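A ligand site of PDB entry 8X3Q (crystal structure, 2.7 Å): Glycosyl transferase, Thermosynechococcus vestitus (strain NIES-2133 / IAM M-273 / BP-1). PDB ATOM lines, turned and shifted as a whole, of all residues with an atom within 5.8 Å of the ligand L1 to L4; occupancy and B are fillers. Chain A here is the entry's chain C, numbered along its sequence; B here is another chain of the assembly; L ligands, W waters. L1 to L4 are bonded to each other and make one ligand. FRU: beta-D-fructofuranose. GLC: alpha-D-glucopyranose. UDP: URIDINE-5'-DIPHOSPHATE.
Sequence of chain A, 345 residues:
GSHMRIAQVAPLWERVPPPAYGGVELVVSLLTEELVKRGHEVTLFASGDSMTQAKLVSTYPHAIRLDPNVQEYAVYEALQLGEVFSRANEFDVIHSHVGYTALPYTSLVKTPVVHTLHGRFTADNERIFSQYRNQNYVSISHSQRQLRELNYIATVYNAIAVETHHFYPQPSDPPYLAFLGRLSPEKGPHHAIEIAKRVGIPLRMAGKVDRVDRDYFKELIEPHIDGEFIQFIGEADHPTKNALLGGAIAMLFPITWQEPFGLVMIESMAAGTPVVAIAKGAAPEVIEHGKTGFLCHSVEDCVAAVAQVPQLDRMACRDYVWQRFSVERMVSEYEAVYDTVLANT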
ATOM      1  N   PRO A  11     -19.647 -20.568  -1.506  1.00  0.00           N
ATOM      2  CA  PRO A  11     -19.059 -21.795  -2.071  1.00  0.00           C
ATOM      3  C   PRO A  11     -18.467 -21.517  -3.437  1.00  0.00           C
ATOM      4  O   PRO A  11     -18.833 -20.561  -4.136  1.00  0.00           O
ATOM      5  CB  PRO A  11     -20.234 -22.774  -2.153  1.00  0.00           C
ATOM      6  CG  PRO A  11     -21.473 -21.950  -1.972  1.00  0.00           C
ATOM      7  CD  PRO A  11     -21.082 -20.716  -1.215  1.00  0.00           C
ATOM      8  N   LEU A  12     -17.528 -22.373  -3.841  1.00  0.00           N
ATOM      9  CA  LEU A  12     -16.755 -22.156  -5.046  1.00  0.00           C
ATOM     10  C   LEU A  12     -17.217 -22.991  -6.225  1.00  0.00           C
ATOM     11  O   LEU A  12     -16.628 -22.893  -7.303  1.00  0.00           O
ATOM     12  CB  LEU A  12     -15.276 -22.431  -4.776  1.00  0.00           C
ATOM     13  CG  LEU A  12     -14.697 -21.506  -3.705  1.00  0.00           C
ATOM     14  CD1 LEU A  12     -13.277 -21.897  -3.321  1.00  0.00           C
ATOM     15  CD2 LEU A  12     -14.758 -20.083  -4.226  1.00  0.00           C
ATOM     16  N   TRP A  13     -18.272 -23.787  -6.055  1.00  0.00           N
ATOM     17  CA  TRP A  13     -18.750 -24.628  -7.151  1.00  0.00           C
ATOM     18  C   TRP A  13     -19.265 -23.783  -8.306  1.00  0.00           C
ATOM     19  O   TRP A  13     -19.129 -24.182  -9.464  1.00  0.00           O
ATOM     20  CB  TRP A  13     -19.839 -25.571  -6.655  1.00  0.00           C
ATOM     21  CG  TRP A  13     -19.330 -26.632  -5.736  1.00  0.00           C
ATOM     22  CD1 TRP A  13     -19.506 -26.707  -4.380  1.00  0.00           C
ATOM     23  CD2 TRP A  13     -18.549 -27.773  -6.097  1.00  0.00           C
ATOM     24  NE1 TRP A  13     -18.883 -27.822  -3.874  1.00  0.00           N
ATOM     25  CE2 TRP A  13     -18.284 -28.502  -4.915  1.00  0.00           C
ATOM     26  CE3 TRP A  13     -18.043 -28.261  -7.310  1.00  0.00           C
ATOM     27  CZ2 TRP A  13     -17.544 -29.677  -4.910  1.00  0.00           C
ATOM     28  CZ3 TRP A  13     -17.311 -29.437  -7.299  1.00  0.00           C
ATOM     29  CH2 TRP A  13     -17.058 -30.129  -6.106  1.00  0.00           C
ATOM     30  N   GLU A  14     -19.844 -22.631  -8.023  1.00  0.00           N
ATOM     31  CA  GLU A  14     -20.437 -21.786  -9.040  1.00  0.00           C
ATOM     32  C   GLU A  14     -19.973 -20.343  -8.897  1.00  0.00           C
ATOM     33  O   GLU A  14     -19.530 -19.907  -7.830  1.00  0.00           O
ATOM     34  CB  GLU A  14     -21.967 -21.832  -8.990  1.00  0.00           C
ATOM     35  CG  GLU A  14     -22.570 -23.190  -9.297  1.00  0.00           C
ATOM     36  CD  GLU A  14     -22.286 -23.633 -10.720  1.00  0.00           C
ATOM     37  OE1 GLU A  14     -22.141 -22.752 -11.607  1.00  0.00           O
ATOM     38  OE2 GLU A  14     -22.211 -24.849 -10.955  1.00  0.00           O
ATOM     39  N   TYR A  21     -26.914 -23.317 -13.483  1.00  0.00           N
ATOM     40  CA  TYR A  21     -27.265 -23.887 -12.190  1.00  0.00           C
ATOM     41  C   TYR A  21     -26.494 -23.207 -11.069  1.00  0.00           C
ATOM     42  O   TYR A  21     -25.331 -22.831 -11.223  1.00  0.00           O
ATOM     43  CB  TYR A  21     -26.980 -25.392 -12.161  1.00  0.00           C
ATOM     44  CG  TYR A  21     -27.286 -26.026 -10.821  1.00  0.00           C
ATOM     45  CD1 TYR A  21     -28.576 -26.420 -10.497  1.00  0.00           C
ATOM     46  CD2 TYR A  21     -26.287 -26.193  -9.868  1.00  0.00           C
ATOM     47  CE1 TYR A  21     -28.864 -26.973  -9.270  1.00  0.00           C
ATOM     48  CE2 TYR A  21     -26.570 -26.746  -8.633  1.00  0.00           C
ATOM     49  CZ  TYR A  21     -27.855 -27.136  -8.337  1.00  0.00           C
ATOM     50  OH  TYR A  21     -28.135 -27.687  -7.115  1.00  0.00           O
ATOM     51  N   GLY A  22     -27.155 -23.037  -9.927  1.00  0.00           N
ATOM     52  CA  GLY A  22     -26.533 -22.461  -8.750  1.00  0.00           C
ATOM     53  C   GLY A  22     -27.523 -21.762  -7.851  1.00  0.00           C
ATOM     54  O   GLY A  22     -28.039 -20.695  -8.192  1.00  0.00           O
ATOM     55  N   GLY A  23     -27.808 -22.363  -6.705  1.00  0.00           N
ATOM     56  CA  GLY A  23     -28.761 -21.799  -5.772  1.00  0.00           C
ATOM     57  C   GLY A  23     -28.134 -20.908  -4.713  1.00  0.00           C
ATOM     58  O   GLY A  23     -28.466 -19.720  -4.633  1.00  0.00           O
ATOM     59  N   VAL A  24     -27.234 -21.465  -3.915  1.00  0.00           N
ATOM     60  CA  VAL A  24     -26.619 -20.713  -2.824  1.00  0.00           C
ATOM     61  C   VAL A  24     -25.861 -19.506  -3.371  1.00  0.00           C
ATOM     62  O   VAL A  24     -25.954 -18.393  -2.828  1.00  0.00           O
ATOM     63  CB  VAL A  24     -25.690 -21.618  -1.996  1.00  0.00           C
ATOM     64  CG1 VAL A  24     -25.000 -20.809  -0.903  1.00  0.00           C
ATOM     65  CG2 VAL A  24     -26.481 -22.774  -1.410  1.00  0.00           C
ATOM     66  N   GLU A  25     -25.103 -19.698  -4.448  1.00  0.00           N
ATOM     67  CA  GLU A  25     -24.338 -18.596  -5.033  1.00  0.00           C
ATOM     68  C   GLU A  25     -25.257 -17.469  -5.468  1.00  0.00           C
ATOM     69  O   GLU A  25     -24.950 -16.286  -5.256  1.00  0.00           O
ATOM     70  CB  GLU A  25     -23.512 -19.111  -6.215  1.00  0.00           C
ATOM     71  CG  GLU A  25     -22.395 -20.052  -5.811  1.00  0.00           C
ATOM     72  CD  GLU A  25     -22.859 -21.496  -5.699  1.00  0.00           C
ATOM     73  OE1 GLU A  25     -21.995 -22.385  -5.567  1.00  0.00           O
ATOM     74  OE2 GLU A  25     -24.087 -21.745  -5.732  1.00  0.00           O
ATOM     75  N   TYR A 100     -20.655 -26.344   7.351  1.00  0.00           N
ATOM     76  CA  TYR A 100     -19.994 -26.672   8.605  1.00  0.00           C
ATOM     77  C   TYR A 100     -18.478 -26.505   8.553  1.00  0.00           C
ATOM     78  O   TYR A 100     -17.842 -26.477   9.604  1.00  0.00           O
ATOM     79  CB  TYR A 100     -20.340 -28.105   9.027  1.00  0.00           C
ATOM     80  CG  TYR A 100     -20.042 -29.169   7.984  1.00  0.00           C
ATOM     81  CD1 TYR A 100     -18.746 -29.643   7.811  1.00  0.00           C
ATOM     82  CD2 TYR A 100     -21.045 -29.689   7.184  1.00  0.00           C
ATOM     83  CE1 TYR A 100     -18.460 -30.613   6.871  1.00  0.00           C
ATOM     84  CE2 TYR A 100     -20.765 -30.658   6.236  1.00  0.00           C
ATOM     85  CZ  TYR A 100     -19.481 -31.116   6.085  1.00  0.00           C
ATOM     86  OH  TYR A 100     -19.202 -32.075   5.138  1.00  0.00           O
ATOM     87  N   HIS A 118     -27.981 -23.442   4.318  1.00  0.00           N
ATOM     88  CA  HIS A 118     -28.580 -23.608   3.008  1.00  0.00           C
ATOM     89  C   HIS A 118     -28.964 -25.043   2.677  1.00  0.00           C
ATOM     90  O   HIS A 118     -29.437 -25.301   1.563  1.00  0.00           O
ATOM     91  CB  HIS A 118     -27.610 -23.098   1.929  1.00  0.00           C
ATOM     92  CG  HIS A 118     -27.541 -21.600   1.826  1.00  0.00           C
ATOM     93  ND1 HIS A 118     -28.357 -20.875   0.987  1.00  0.00           N
ATOM     94  CD2 HIS A 118     -26.726 -20.700   2.440  1.00  0.00           C
ATOM     95  CE1 HIS A 118     -28.064 -19.595   1.098  1.00  0.00           C
ATOM     96  NE2 HIS A 118     -27.082 -19.455   1.971  1.00  0.00           N
ATOM     97  N   GLY A 119     -28.783 -25.984   3.614  1.00  0.00           N
ATOM     98  CA  GLY A 119     -28.866 -27.393   3.285  1.00  0.00           C
ATOM     99  C   GLY A 119     -29.651 -28.219   4.290  1.00  0.00           C
ATOM    100  O   GLY A 119     -29.904 -27.817   5.419  1.00  0.00           O
ATOM    101  N   ARG A 120     -30.016 -29.407   3.825  1.00  0.00           N
ATOM    102  CA  ARG A 120     -30.655 -30.427   4.661  1.00  0.00           C
ATOM    103  C   ARG A 120     -29.729 -30.856   5.808  1.00  0.00           C
ATOM    104  O   ARG A 120     -28.499 -30.819   5.708  1.00  0.00           O
ATOM    105  CB  ARG A 120     -31.025 -31.629   3.783  1.00  0.00           C
ATOM    106  CG  ARG A 120     -31.659 -32.848   4.474  1.00  0.00           C
ATOM    107  CD  ARG A 120     -32.054 -33.994   3.485  1.00  0.00           C
ATOM    108  NE  ARG A 120     -30.935 -34.634   2.796  1.00  0.00           N
ATOM    109  CZ  ARG A 120     -30.296 -35.707   3.247  1.00  0.00           C
ATOM    110  NH1 ARG A 120     -30.647 -36.273   4.394  1.00  0.00           N
ATOM    111  NH2 ARG A 120     -29.289 -36.212   2.539  1.00  0.00           N
ATOM    112  N   THR A 122     -28.329 -33.913   8.043  1.00  0.00           N
ATOM    113  CA  THR A 122     -28.054 -35.313   7.798  1.00  0.00           C
ATOM    114  C   THR A 122     -27.589 -35.979   9.079  1.00  0.00           C
ATOM    115  O   THR A 122     -27.274 -35.330  10.073  1.00  0.00           O
ATOM    116  CB  THR A 122     -26.996 -35.494   6.698  1.00  0.00           C
ATOM    117  OG1 THR A 122     -25.826 -34.737   7.017  1.00  0.00           O
ATOM    118  CG2 THR A 122     -27.560 -35.036   5.390  1.00  0.00           C
ATOM    119  N   ARG A 182     -31.757 -29.682 -10.927  1.00  0.00           N
ATOM    120  CA  ARG A 182     -30.769 -30.741 -11.117  1.00  0.00           C
ATOM    121  C   ARG A 182     -31.461 -32.094 -11.191  1.00  0.00           C
ATOM    122  O   ARG A 182     -32.443 -32.349 -10.493  1.00  0.00           O
ATOM    123  CB  ARG A 182     -29.746 -30.712  -9.979  1.00  0.00           C
ATOM    124  CG  ARG A 182     -30.248 -31.400  -8.728  1.00  0.00           C
ATOM    125  CD  ARG A 182     -29.548 -30.974  -7.462  1.00  0.00           C
ATOM    126  NE  ARG A 182     -30.062 -31.744  -6.345  1.00  0.00           N
ATOM    127  CZ  ARG A 182     -29.854 -31.445  -5.069  1.00  0.00           C
ATOM    128  NH1 ARG A 182     -29.144 -30.376  -4.743  1.00  0.00           N
ATOM    129  NH2 ARG A 182     -30.357 -32.217  -4.119  1.00  0.00           N
ATOM    130  N   SER A 184     -31.801 -35.013 -10.022  1.00  0.00           N
ATOM    131  CA  SER A 184     -31.500 -35.719  -8.778  1.00  0.00           C
ATOM    132  C   SER A 184     -32.743 -36.399  -8.235  1.00  0.00           C
ATOM    133  O   SER A 184     -33.857 -35.887  -8.379  1.00  0.00           O
ATOM    134  CB  SER A 184     -30.956 -34.743  -7.726  1.00  0.00           C
ATOM    135  OG  SER A 184     -30.711 -35.373  -6.472  1.00  0.00           O
ATOM    136  N   GLU A 186     -33.686 -36.396  -5.429  1.00  0.00           N
ATOM    137  CA  GLU A 186     -34.228 -35.520  -4.371  1.00  0.00           C
ATOM    138  C   GLU A 186     -35.216 -34.551  -4.993  1.00  0.00           C
ATOM    139  O   GLU A 186     -36.067 -34.045  -4.271  1.00  0.00           O
ATOM    140  CB  GLU A 186     -33.023 -34.893  -3.675  1.00  0.00           C
ATOM    141  CG  GLU A 186     -32.110 -35.919  -3.055  1.00  0.00           C
ATOM    142  CD  GLU A 186     -31.163 -35.307  -2.037  1.00  0.00           C
ATOM    143  OE1 GLU A 186     -30.896 -34.111  -2.173  1.00  0.00           O
ATOM    144  OE2 GLU A 186     -30.716 -36.016  -1.125  1.00  0.00           O
ATOM    145  N   LYS A 208     -28.985 -29.625 -14.827  1.00  0.00           N
ATOM    146  CA  LYS A 208     -27.722 -30.335 -14.940  1.00  0.00           C
ATOM    147  C   LYS A 208     -27.853 -31.773 -14.435  1.00  0.00           C
ATOM    148  O   LYS A 208     -28.736 -32.098 -13.628  1.00  0.00           O
ATOM    149  CB  LYS A 208     -26.624 -29.608 -14.172  1.00  0.00           C
ATOM    150  CG  LYS A 208     -26.891 -29.481 -12.672  1.00  0.00           C
ATOM    151  CD  LYS A 208     -25.597 -29.463 -11.880  1.00  0.00           C
ATOM    152  CE  LYS A 208     -25.857 -29.717 -10.411  1.00  0.00           C
ATOM    153  NZ  LYS A 208     -24.601 -29.624  -9.597  1.00  0.00           N
ATOM    154  N   ASP A 210     -25.110 -33.861 -12.709  1.00  0.00           N
ATOM    155  CA  ASP A 210     -23.751 -33.796 -12.225  1.00  0.00           C
ATOM    156  C   ASP A 210     -23.235 -35.177 -11.830  1.00  0.00           C
ATOM    157  O   ASP A 210     -23.927 -36.194 -11.968  1.00  0.00           O
ATOM    158  CB  ASP A 210     -23.631 -32.782 -11.084  1.00  0.00           C
ATOM    159  CG  ASP A 210     -24.205 -33.292  -9.778  1.00  0.00           C
ATOM    160  OD1 ASP A 210     -24.991 -34.258  -9.785  1.00  0.00           O
ATOM    161  OD2 ASP A 210     -23.854 -32.709  -8.730  1.00  0.00           O
ATOM    162  N   VAL A 212     -22.653 -37.074  -9.304  1.00  0.00           N
ATOM    163  CA  VAL A 212     -23.280 -38.017  -8.371  1.00  0.00           C
ATOM    164  C   VAL A 212     -24.594 -38.597  -8.852  1.00  0.00           C
ATOM    165  O   VAL A 212     -25.055 -39.589  -8.270  1.00  0.00           O
ATOM    166  CB  VAL A 212     -23.496 -37.346  -6.997  1.00  0.00           C
ATOM    167  CG1 VAL A 212     -22.174 -36.906  -6.400  1.00  0.00           C
ATOM    168  CG2 VAL A 212     -24.447 -36.178  -7.138  1.00  0.00           C
ATOM    169  N   ASP A 213     -25.212 -38.037  -9.881  1.00  0.00           N
ATOM    170  CA  ASP A 213     -26.514 -38.507 -10.348  1.00  0.00           C
ATOM    171  C   ASP A 213     -26.465 -39.119 -11.735  1.00  0.00           C
ATOM    172  O   ASP A 213     -27.514 -39.306 -12.359  1.00  0.00           O
ATOM    173  CB  ASP A 213     -27.541 -37.358 -10.353  1.00  0.00           C
ATOM    174  CG  ASP A 213     -27.452 -36.494  -9.121  1.00  0.00           C
ATOM    175  OD1 ASP A 213     -27.379 -37.036  -8.008  1.00  0.00           O
ATOM    176  OD2 ASP A 213     -27.496 -35.252  -9.270  1.00  0.00           O
ATOM    177  N   TRP A 257     -37.741 -35.421  -0.785  1.00  0.00           N
ATOM    178  CA  TRP A 257     -36.575 -34.944  -0.065  1.00  0.00           C
ATOM    179  C   TRP A 257     -36.997 -33.828   0.898  1.00  0.00           C
ATOM    180  O   TRP A 257     -37.980 -33.125   0.660  1.00  0.00           O
ATOM    181  CB  TRP A 257     -35.537 -34.458  -1.084  1.00  0.00           C
ATOM    182  CG  TRP A 257     -34.343 -33.740  -0.578  1.00  0.00           C
ATOM    183  CD1 TRP A 257     -33.495 -34.150   0.404  1.00  0.00           C
ATOM    184  CD2 TRP A 257     -33.831 -32.495  -1.061  1.00  0.00           C
ATOM    185  NE1 TRP A 257     -32.490 -33.229   0.561  1.00  0.00           N
ATOM    186  CE2 TRP A 257     -32.674 -32.196  -0.317  1.00  0.00           C
ATOM    187  CE3 TRP A 257     -34.245 -31.598  -2.050  1.00  0.00           C
ATOM    188  CZ2 TRP A 257     -31.927 -31.045  -0.532  1.00  0.00           C
ATOM    189  CZ3 TRP A 257     -33.500 -30.449  -2.251  1.00  0.00           C
ATOM    190  CH2 TRP A 257     -32.357 -30.183  -1.501  1.00  0.00           C
ATOM    191  N   GLN B  71     -21.459 -41.119   5.303  1.00  0.00           N
ATOM    192  CA  GLN B  71     -21.347 -40.650   3.933  1.00  0.00           C
ATOM    193  C   GLN B  71     -20.536 -39.374   3.796  1.00  0.00           C
ATOM    194  O   GLN B  71     -20.163 -39.013   2.674  1.00  0.00           O
ATOM    195  CB  GLN B  71     -22.752 -40.427   3.339  1.00  0.00           C
ATOM    196  CG  GLN B  71     -23.345 -41.650   2.649  1.00  0.00           C
ATOM    197  CD  GLN B  71     -23.681 -42.755   3.621  1.00  0.00           C
ATOM    198  OE1 GLN B  71     -23.175 -43.872   3.513  1.00  0.00           O
ATOM    199  NE2 GLN B  71     -24.551 -42.463   4.578  1.00  0.00           N
ATOM    200  N   GLU B  72     -20.248 -38.685   4.909  1.00  0.00           N
ATOM    201  CA  GLU B  72     -19.565 -37.402   4.911  1.00  0.00           C
ATOM    202  C   GLU B  72     -18.369 -37.479   5.858  1.00  0.00           C
ATOM    203  O   GLU B  72     -18.491 -37.198   7.055  1.00  0.00           O
ATOM    204  CB  GLU B  72     -20.523 -36.281   5.293  1.00  0.00           C
ATOM    205  CG  GLU B  72     -21.781 -36.226   4.447  1.00  0.00           C
ATOM    206  CD  GLU B  72     -22.776 -35.186   4.932  1.00  0.00           C
ATOM    207  OE1 GLU B  72     -23.894 -35.589   5.345  1.00  0.00           O
ATOM    208  OE2 GLU B  72     -22.446 -33.982   4.912  1.00  0.00           O
HETATM  209  C1  FRU L   1     -27.497 -32.349  -1.593  1.00  0.00           C
HETATM  210  C2  FRU L   1     -26.543 -32.845  -0.460  1.00  0.00           C
HETATM  211  C3  FRU L   1     -25.849 -33.832  -0.941  1.00  0.00           C
HETATM  212  C4  FRU L   1     -25.932 -34.989   0.048  1.00  0.00           C
HETATM  213  C5  FRU L   1     -26.914 -34.538   1.159  1.00  0.00           C
HETATM  214  C6  FRU L   1     -26.147 -34.302   2.506  1.00  0.00           C
HETATM  215  O1  FRU L   1     -28.659 -33.139  -1.580  1.00  0.00           O
HETATM  216  O2  FRU L   1     -25.675 -31.835   0.067  1.00  0.00           O
HETATM  217  O3  FRU L   1     -24.408 -33.417  -1.123  1.00  0.00           O
HETATM  218  O4  FRU L   1     -26.458 -36.100  -0.544  1.00  0.00           O
HETATM  219  O5  FRU L   1     -27.451 -33.449   0.737  1.00  0.00           O
HETATM  220  O6  FRU L   1     -25.069 -35.184   2.650  1.00  0.00           O
HETATM  221  C1  GLC L   2     -26.008 -30.504  -0.288  1.00  0.00           C
HETATM  222  C2  GLC L   2     -24.926 -29.950  -1.147  1.00  0.00           C
HETATM  223  C3  GLC L   2     -23.648 -30.027  -0.463  1.00  0.00           C
HETATM  224  C4  GLC L   2     -23.642 -29.383   0.889  1.00  0.00           C
HETATM  225  C5  GLC L   2     -25.010 -28.916   1.500  1.00  0.00           C
HETATM  226  C6  GLC L   2     -25.156 -27.505   1.378  1.00  0.00           C
HETATM  227  O2  GLC L   2     -24.990 -30.717  -2.460  1.00  0.00           O
HETATM  228  O3  GLC L   2     -22.566 -29.347  -1.212  1.00  0.00           O
HETATM  229  O4  GLC L   2     -23.053 -30.313   1.803  1.00  0.00           O
HETATM  230  O5  GLC L   2     -26.223 -29.664   0.920  1.00  0.00           O
HETATM  231  O6  GLC L   2     -26.202 -27.220   0.482  1.00  0.00           O
HETATM  232  C1  GLC L   3     -24.265 -30.093  -3.505  1.00  0.00           C
HETATM  233  C2  GLC L   3     -25.131 -29.333  -4.464  1.00  0.00           C
HETATM  234  C3  GLC L   3     -25.854 -30.179  -5.417  1.00  0.00           C
HETATM  235  C4  GLC L   3     -24.996 -31.218  -6.051  1.00  0.00           C
HETATM  236  C5  GLC L   3     -24.324 -32.105  -4.983  1.00  0.00           C
HETATM  237  C6  GLC L   3     -23.512 -33.080  -5.592  1.00  0.00           C
HETATM  238  O2  GLC L   3     -26.132 -28.463  -3.748  1.00  0.00           O
HETATM  239  O3  GLC L   3     -26.393 -29.319  -6.494  1.00  0.00           O
HETATM  240  O4  GLC L   3     -25.794 -32.033  -6.924  1.00  0.00           O
HETATM  241  O5  GLC L   3     -23.456 -31.146  -4.144  1.00  0.00           O
HETATM  242  O6  GLC L   3     -23.003 -33.921  -4.590  1.00  0.00           O
HETATM  243  C1  GLC L   4     -25.551 -27.295  -3.165  1.00  0.00           C
HETATM  244  C2  GLC L   4     -26.590 -26.219  -3.048  1.00  0.00           C
HETATM  245  C3  GLC L   4     -26.778 -25.478  -4.256  1.00  0.00           C
HETATM  246  C4  GLC L   4     -25.513 -24.851  -4.711  1.00  0.00           C
HETATM  247  C5  GLC L   4     -24.427 -25.920  -5.030  1.00  0.00           C
HETATM  248  C6  GLC L   4     -23.169 -25.270  -5.197  1.00  0.00           C
HETATM  249  O2  GLC L   4     -27.888 -26.861  -2.646  1.00  0.00           O
HETATM  250  O3  GLC L   4     -27.783 -24.419  -4.018  1.00  0.00           O
HETATM  251  O4  GLC L   4     -25.745 -24.089  -5.887  1.00  0.00           O
HETATM  252  O5  GLC L   4     -24.312 -26.896  -3.856  1.00  0.00           O
HETATM  253  O6  GLC L   4     -22.789 -24.726  -3.954  1.00  0.00           O
HETATM  254  N1  UDP L   5     -30.996 -23.474 -12.066  1.00  0.00           N
HETATM  255  C2  UDP L   5     -30.763 -23.109 -13.359  1.00  0.00           C
HETATM  256  N3  UDP L   5     -30.750 -23.918 -14.314  1.00  0.00           N
HETATM  257  C4  UDP L   5     -30.946 -25.128 -14.241  1.00  0.00           C
HETATM  258  C5  UDP L   5     -31.208 -25.762 -13.126  1.00  0.00           C
HETATM  259  C6  UDP L   5     -31.239 -24.894 -11.981  1.00  0.00           C
HETATM  260  O2  UDP L   5     -30.547 -21.963 -13.587  1.00  0.00           O
HETATM  261  O4  UDP L   5     -30.906 -25.753 -15.245  1.00  0.00           O
HETATM  262  C1' UDP L   5     -31.023 -22.586 -10.983  1.00  0.00           C
HETATM  263  C2' UDP L   5     -32.398 -22.473 -10.451  1.00  0.00           C
HETATM  264  O2' UDP L   5     -33.139 -21.471 -11.204  1.00  0.00           O
HETATM  265  C3' UDP L   5     -32.239 -22.074  -9.071  1.00  0.00           C
HETATM  266  C4' UDP L   5     -30.991 -22.738  -8.608  1.00  0.00           C
HETATM  267  O4' UDP L   5     -30.168 -23.073  -9.830  1.00  0.00           O
HETATM  268  O3' UDP L   5     -32.073 -20.627  -8.990  1.00  0.00           O
HETATM  269  C5' UDP L   5     -31.315 -23.976  -7.877  1.00  0.00           C
HETATM  270  O5' UDP L   5     -31.817 -23.662  -6.598  1.00  0.00           O
HETATM  271  PA  UDP L   5     -32.814 -24.748  -5.863  1.00  0.00           P
HETATM  272  O1A UDP L   5     -32.981 -24.435  -4.449  1.00  0.00           O
HETATM  273  O2A UDP L   5     -34.183 -24.641  -6.347  1.00  0.00           O
HETATM  274  O3A UDP L   5     -32.216 -26.272  -6.100  1.00  0.00           O
HETATM  275  PB  UDP L   5     -31.067 -26.983  -5.160  1.00  0.00           P
HETATM  276  O1B UDP L   5     -31.617 -27.473  -3.904  1.00  0.00           O
HETATM  277  O2B UDP L   5     -30.087 -25.996  -4.675  1.00  0.00           O
HETATM  278  O3B UDP L   5     -30.319 -28.193  -5.992  1.00  0.00           O
HETATM  279  O   HOH W   1     -25.086 -36.471  -3.036  1.00  0.00           O
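An oxygen (O3) of GLC L3 is in hydrogen-bond range of the side-chain hydroxyl (OH) of Tyr 21 (2.5 Å). O1 of FRU L1 lies within hydrogen-bond range of OE1 of Glu 186 (2.5 Å). OD2 of Asp 210 is in hydrogen-bond range of O4 of GLC L3. The backbone NH of Gly 23 lies within hydrogen-bond range of an oxygen (O4) of GLC L4, 2.8 Å away. An oxygen (O4) of GLC L4 sits at hydrogen-bond distance from the side-chain carboxylate (OE2) of Glu 25, 2.9 Å away. The side-chain carboxylate of Glu 72 of chain B sits at hydrogen-bond distance from an oxygen (O6) of FRU L1 (3.0 Å). The backbone NH (N) of Val 24 sits at hydrogen-bond distance from an oxygen (O3) of GLC L4, 3.0 Å away. NH2 of Arg 182 lies within hydrogen-bond range of O1 of FRU L1, at 3.2 Å. OH of Tyr 21 sits at hydrogen-bond distance from O3B of UDP L5, at 2.5 Å. The guanidinium group (NH1) of Arg 182 is in salt-bridge range of an oxygen (O3B) of UDP L5 (2.8 Å). The backbone NH (N) of Gly 22 lies within hydrogen-bond range of an oxygen (O4') of UDP L5.
An oxygen (O3) of GLC L4 is in hydrogen-bond range of an oxygen (O2B) of UDP L5 (2.9 Å).
NH2 of Arg 182 is in salt-bridge range of OE1 of Glu 186, at 2.8 Å. The side-chain carboxylate (OE2) of Glu 186 lies within salt-bridge range of the guanidinium group (NH2) of Arg 120 (3.9 Å). NE1 of Trp 257 sits close to OE1 of Glu 186, 3.3 Å away. N of Glu 186 sits close to OG of Ser 184. The side-chain carboxylate (OD2) of Asp 210 is in salt-bridge range of the side-chain amino group (NZ) of Lys 208 (3.3 Å). OD1 of Asp 210 sits close to OD2 of Asp 213 (2.7 Å). OE1 of Glu 25 is in hydrogen-bond range of N of Glu 14 (3.3 Å). The side-chain hydroxyl (OG1) of Thr 122 sits at hydrogen-bond distance from the side-chain carboxylate (OE1) of Glu 72 of chain B, at 2.7 Å.
Pro 11 touches the ligand L1 to L4. CB of Trp 13 touches C6 of GLC L4, 3.6 Å away. Gly 22 touches the ligand L1 to L4. O of His 118 touches O6 of GLC L2 (3.9 Å). CA of Gly 119 touches O6 of GLC L2 (3.9 Å). NH2 of Arg 120 touches C5 of FRU L1 (3.2 Å). Thr 122 touches the ligand L1 to L4. NZ of Lys 208 touches O3 of GLC L3, at 3.6 Å. CG2 of Val 212 touches C6 of GLC L3, at 3.6 Å. Hydrophobic or aromatic side chains that line the ligand L1 to L4: Pro 11, Trp 13, Tyr 21, Val 24 and Val 212. Within 4 Å of the ligand L1 to L4: Pro 11, Trp 13, Tyr 21, Gly 22, Gly 23, Val 24, Glu 25, His 118, Gly 119, Arg 120, Thr 122, Arg 182, Glu 186, Lys 208, Asp 210, Val 212 and Glu 72 of chain B. Along chain A the residues within 4 Å of the ligand L1 to L4 span positions 11 to 212. The nearest printed residue that does not touch the ligand L1 to L4 is Trp 257 (4.02 Å).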
